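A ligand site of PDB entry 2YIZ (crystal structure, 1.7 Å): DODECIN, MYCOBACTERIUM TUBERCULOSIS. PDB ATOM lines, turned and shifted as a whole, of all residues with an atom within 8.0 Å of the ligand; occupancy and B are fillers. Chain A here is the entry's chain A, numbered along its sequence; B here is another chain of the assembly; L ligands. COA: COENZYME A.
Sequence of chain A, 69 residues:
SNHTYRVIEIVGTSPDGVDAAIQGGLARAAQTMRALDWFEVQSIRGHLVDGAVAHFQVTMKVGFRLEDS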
ATOM      1  N   THR A   4       3.068  17.328  33.615  1.00  0.00           N
ATOM      2  CA  THR A   4       2.419  16.506  32.600  1.00  0.00           C
ATOM      3  C   THR A   4       3.083  16.850  31.285  1.00  0.00           C
ATOM      4  O   THR A   4       3.392  18.015  31.035  1.00  0.00           O
ATOM      5  CB  THR A   4       0.918  16.799  32.513  1.00  0.00           C
ATOM      6  OG1 THR A   4       0.305  16.604  33.801  1.00  0.00           O
ATOM      7  CG2 THR A   4       0.251  15.950  31.446  1.00  0.00           C
ATOM      8  N   ARG A   6       3.227  16.256  26.891  1.00  0.00           N
ATOM      9  CA  ARG A   6       2.504  15.898  25.677  1.00  0.00           C
ATOM     10  C   ARG A   6       3.526  15.356  24.681  1.00  0.00           C
ATOM     11  O   ARG A   6       4.647  15.849  24.601  1.00  0.00           O
ATOM     12  CB  ARG A   6       1.771  17.111  25.106  1.00  0.00           C
ATOM     13  CG  ARG A   6       1.128  16.880  23.739  1.00  0.00           C
ATOM     14  CD  ARG A   6      -0.333  16.594  23.764  1.00  0.00           C
ATOM     15  NE  ARG A   6      -0.837  16.504  22.389  1.00  0.00           N
ATOM     16  CZ  ARG A   6      -1.466  17.456  21.718  1.00  0.00           C
ATOM     17  NH1 ARG A   6      -1.791  18.622  22.293  1.00  0.00           N
ATOM     18  NH2 ARG A   6      -1.828  17.232  20.446  1.00  0.00           N
ATOM     19  N   ALA A  29      10.131  21.845  14.610  1.00  0.00           N
ATOM     20  CA  ALA A  29       9.258  21.695  15.774  1.00  0.00           C
ATOM     21  C   ALA A  29       9.530  22.811  16.795  1.00  0.00           C
ATOM     22  O   ALA A  29       8.581  23.368  17.387  1.00  0.00           O
ATOM     23  CB  ALA A  29       9.422  20.292  16.410  1.00  0.00           C
ATOM     24  N   THR A  32       7.767  26.607  16.709  1.00  0.00           N
ATOM     25  CA  THR A  32       6.414  26.876  17.216  1.00  0.00           C
ATOM     26  C   THR A  32       6.111  26.242  18.573  1.00  0.00           C
ATOM     27  O   THR A  32       5.164  26.677  19.243  1.00  0.00           O
ATOM     28  CB  THR A  32       5.356  26.437  16.194  1.00  0.00           C
ATOM     29  OG1 THR A  32       5.587  25.082  15.806  1.00  0.00           O
ATOM     30  CG2 THR A  32       5.402  27.344  14.951  1.00  0.00           C
ATOM     31  N   MET A  33       6.896  25.262  19.007  1.00  0.00           N
ATOM     32  CA  MET A  33       6.656  24.585  20.287  1.00  0.00           C
ATOM     33  C   MET A  33       7.630  25.024  21.360  1.00  0.00           C
ATOM     34  O   MET A  33       8.716  25.547  21.065  1.00  0.00           O
ATOM     35  CB  MET A  33       6.793  23.098  20.115  1.00  0.00           C
ATOM     36  CG  MET A  33       5.948  22.554  19.015  1.00  0.00           C
ATOM     37  SD  MET A  33       6.553  20.938  18.676  1.00  0.00           S
ATOM     38  CE  MET A  33       6.098  20.115  20.203  1.00  0.00           C
ATOM     39  N   ARG A  34       7.231  24.806  22.612  1.00  0.00           N
ATOM     40  CA  ARG A  34       8.009  25.238  23.745  1.00  0.00           C
ATOM     41  C   ARG A  34       8.241  24.077  24.680  1.00  0.00           C
ATOM     42  O   ARG A  34       7.433  23.145  24.732  1.00  0.00           O
ATOM     43  CB  ARG A  34       7.276  26.364  24.468  1.00  0.00           C
ATOM     44  CG  ARG A  34       7.069  27.617  23.601  1.00  0.00           C
ATOM     45  CD  ARG A  34       6.189  28.651  24.294  1.00  0.00           C
ATOM     46  NE  ARG A  34       4.830  28.162  24.495  1.00  0.00           N
ATOM     47  CZ  ARG A  34       3.857  28.175  23.575  1.00  0.00           C
ATOM     48  NH1 ARG A  34       4.081  28.647  22.349  1.00  0.00           N
ATOM     49  NH2 ARG A  34       2.655  27.698  23.886  1.00  0.00           N
ATOM     50  N   ALA A  35       9.350  24.149  25.421  1.00  0.00           N
ATOM     51  CA  ALA A  35       9.642  23.212  26.495  1.00  0.00           C
ATOM     52  C   ALA A  35       9.850  21.805  25.931  1.00  0.00           C
ATOM     53  O   ALA A  35       9.468  20.813  26.564  1.00  0.00           O
ATOM     54  CB  ALA A  35       8.526  23.222  27.549  1.00  0.00           C
ATOM     55  N   LEU A  36      10.437  21.711  24.739  1.00  0.00           N
ATOM     56  CA  LEU A  36      10.811  20.387  24.180  1.00  0.00           C
ATOM     57  C   LEU A  36      11.826  19.707  25.098  1.00  0.00           C
ATOM     58  O   LEU A  36      12.753  20.340  25.601  1.00  0.00           O
ATOM     59  CB  LEU A  36      11.420  20.518  22.779  1.00  0.00           C
ATOM     60  CG  LEU A  36      10.556  21.081  21.649  1.00  0.00           C
ATOM     61  CD1 LEU A  36      11.319  20.922  20.323  1.00  0.00           C
ATOM     62  CD2 LEU A  36       9.197  20.414  21.543  1.00  0.00           C
ATOM     63  N   PHE A  64       7.212  17.119  25.229  1.00  0.00           N
ATOM     64  CA  PHE A  64       7.402  18.460  25.792  1.00  0.00           C
ATOM     65  C   PHE A  64       6.534  18.669  27.017  1.00  0.00           C
ATOM     66  O   PHE A  64       5.515  18.041  27.189  1.00  0.00           O
ATOM     67  CB  PHE A  64       7.153  19.549  24.743  1.00  0.00           C
ATOM     68  CG  PHE A  64       5.744  19.594  24.180  1.00  0.00           C
ATOM     69  CD1 PHE A  64       5.411  18.854  23.054  1.00  0.00           C
ATOM     70  CD2 PHE A  64       4.779  20.386  24.764  1.00  0.00           C
ATOM     71  CE1 PHE A  64       4.116  18.927  22.517  1.00  0.00           C
ATOM     72  CE2 PHE A  64       3.491  20.447  24.233  1.00  0.00           C
ATOM     73  CZ  PHE A  64       3.179  19.713  23.112  1.00  0.00           C
ATOM     74  N   ARG A  65       6.967  19.564  27.891  1.00  0.00           N
ATOM     75  CA  ARG A  65       6.254  19.812  29.098  1.00  0.00           C
ATOM     76  C   ARG A  65       5.058  20.734  28.870  1.00  0.00           C
ATOM     77  O   ARG A  65       5.215  21.848  28.328  1.00  0.00           O
ATOM     78  CB  ARG A  65       7.166  20.432  30.143  1.00  0.00           C
ATOM     79  CG  ARG A  65       6.513  20.390  31.506  1.00  0.00           C
ATOM     80  CD  ARG A  65       6.756  21.576  32.314  1.00  0.00           C
ATOM     81  NE  ARG A  65       8.115  21.688  32.806  1.00  0.00           N
ATOM     82  CZ  ARG A  65       8.960  22.687  32.508  1.00  0.00           C
ATOM     83  NH1 ARG A  65       8.644  23.663  31.644  1.00  0.00           N
ATOM     84  NH2 ARG A  65      10.159  22.702  33.087  1.00  0.00           N
ATOM     85  N   LEU A  66       3.887  20.312  29.337  1.00  0.00           N
ATOM     86  CA  LEU A  66       2.705  21.156  29.265  1.00  0.00           C
ATOM     87  C   LEU A  66       2.748  22.266  30.316  1.00  0.00           C
ATOM     88  O   LEU A  66       3.080  22.045  31.489  1.00  0.00           O
ATOM     89  CB  LEU A  66       1.419  20.367  29.488  1.00  0.00           C
ATOM     90  CG  LEU A  66       1.009  19.445  28.357  1.00  0.00           C
ATOM     91  CD1 LEU A  66      -0.246  18.684  28.809  1.00  0.00           C
ATOM     92  CD2 LEU A  66       0.738  20.231  27.084  1.00  0.00           C
ATOM     93  N   GLU A  67       2.355  23.453  29.867  1.00  0.00           N
ATOM     94  CA  GLU A  67       2.213  24.584  30.725  1.00  0.00           C
ATOM     95  C   GLU A  67       0.897  24.397  31.481  1.00  0.00           C
ATOM     96  O   GLU A  67       0.006  23.660  31.029  1.00  0.00           O
ATOM     97  CB  GLU A  67       2.193  25.861  29.865  1.00  0.00           C
ATOM     98  CG  GLU A  67       3.454  26.038  28.986  1.00  0.00           C
ATOM     99  CD  GLU A  67       3.268  26.935  27.751  1.00  0.00           C
ATOM    100  OE1 GLU A  67       2.105  27.198  27.341  1.00  0.00           O
ATOM    101  OE2 GLU A  67       4.290  27.362  27.161  1.00  0.00           O
ATOM    102  N   ASP A  68       0.779  25.032  32.629  1.00  0.00           N
ATOM    103  CA  ASP A  68      -0.461  24.969  33.418  1.00  0.00           C
ATOM    104  C   ASP A  68      -1.579  25.795  32.774  1.00  0.00           C
ATOM    105  O   ASP A  68      -2.606  25.249  32.356  1.00  0.00           O
ATOM    106  CB  ASP A  68      -0.194  25.441  34.849  1.00  0.00           C
ATOM    107  CG  ASP A  68       0.771  24.518  35.593  1.00  0.00           C
ATOM    108  OD1 ASP A  68       0.880  23.335  35.217  1.00  0.00           O
ATOM    109  OD2 ASP A  68       1.427  24.989  36.548  1.00  0.00           O
ATOM    110  N   ARG B  28      -5.028  16.822  34.156  1.00  0.00           N
ATOM    111  CA  ARG B  28      -4.474  17.929  33.380  1.00  0.00           C
ATOM    112  C   ARG B  28      -5.115  17.948  31.997  1.00  0.00           C
ATOM    113  O   ARG B  28      -5.517  19.012  31.504  1.00  0.00           O
ATOM    114  CB  ARG B  28      -2.943  17.826  33.249  1.00  0.00           C
ATOM    115  CG  ARG B  28      -2.307  18.871  32.331  1.00  0.00           C
ATOM    116  CD  ARG B  28      -2.614  20.304  32.793  1.00  0.00           C
ATOM    117  NE  ARG B  28      -2.128  21.287  31.836  1.00  0.00           N
ATOM    118  CZ  ARG B  28      -2.719  21.604  30.686  1.00  0.00           C
ATOM    119  NH1 ARG B  28      -3.846  21.008  30.306  1.00  0.00           N
ATOM    120  NH2 ARG B  28      -2.176  22.509  29.888  1.00  0.00           N
ATOM    121  N   THR B  32      -8.279  21.187  29.592  1.00  0.00           N
ATOM    122  CA  THR B  32      -8.278  21.872  28.290  1.00  0.00           C
ATOM    123  C   THR B  32      -8.773  21.010  27.128  1.00  0.00           C
ATOM    124  O   THR B  32      -8.638  21.399  25.952  1.00  0.00           O
ATOM    125  CB  THR B  32      -6.858  22.394  27.969  1.00  0.00           C
ATOM    126  OG1 THR B  32      -5.925  21.304  28.056  1.00  0.00           O
ATOM    127  CG2 THR B  32      -6.463  23.499  28.944  1.00  0.00           C
HETATM  128  N1A COA L   1       2.451  23.730  26.738  1.00  0.00           N
HETATM  129  C2A COA L   1       1.118  23.821  26.347  1.00  0.00           C
HETATM  130  N3A COA L   1       0.805  24.145  25.030  1.00  0.00           N
HETATM  131  C4A COA L   1       1.813  24.401  24.149  1.00  0.00           C
HETATM  132  C5A COA L   1       3.160  24.314  24.532  1.00  0.00           C
HETATM  133  C6A COA L   1       3.481  23.967  25.846  1.00  0.00           C
HETATM  134  N6A COA L   1       4.724  23.550  26.129  1.00  0.00           N
HETATM  135  N7A COA L   1       3.931  24.605  23.459  1.00  0.00           N
HETATM  136  C8A COA L   1       3.121  24.875  22.408  1.00  0.00           C
HETATM  137  N9A COA L   1       1.805  24.753  22.810  1.00  0.00           N
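The backbone carbonyl oxygen (O) of Arg 65 sits at hydrogen-bond distance from a nitrogen (N6A) of the ligand.
A nitrogen (N1A) of the ligand is in hydrogen-bond range of the backbone NH of Glu 67 (3.1 Å).
A nitrogen (N7A) of the ligand is in hydrogen-bond range of the backbone NH (N) of Arg 34, 3.4 Å away.
O of Arg 34 sits at hydrogen-bond distance from N6A of the ligand, 3.1 Å away.
A nitrogen (N9A) of the ligand lies close to the guanidinium group of Arg 34 (3.2 Å).
N of Leu 66 is in hydrogen-bond range of O of Thr 4 (2.9 Å).
OE2 of Glu 67 is in salt-bridge range of NE of Arg 34 (2.8 Å).
The backbone NH (N) of Arg 65 is in hydrogen-bond range of the backbone carbonyl oxygen (O) of Ala 35 (3.1 Å).
O of Phe 64 is in hydrogen-bond range of N of Arg 6.
NH2 of Arg 28 of chain B sits at hydrogen-bond distance from O of Glu 67 (2.7 Å).
Phe 64 touches the ligand (CD2 to N6A, 3.4 Å).
CA of Leu 66 touches N1A of the ligand (3.6 Å).
Within 4 Å of the ligand: Arg 34, Phe 64, Arg 65, Leu 66 and Glu 67.
The nearest printed residue that does not touch the ligand is Ala 35 (4.1 Å).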
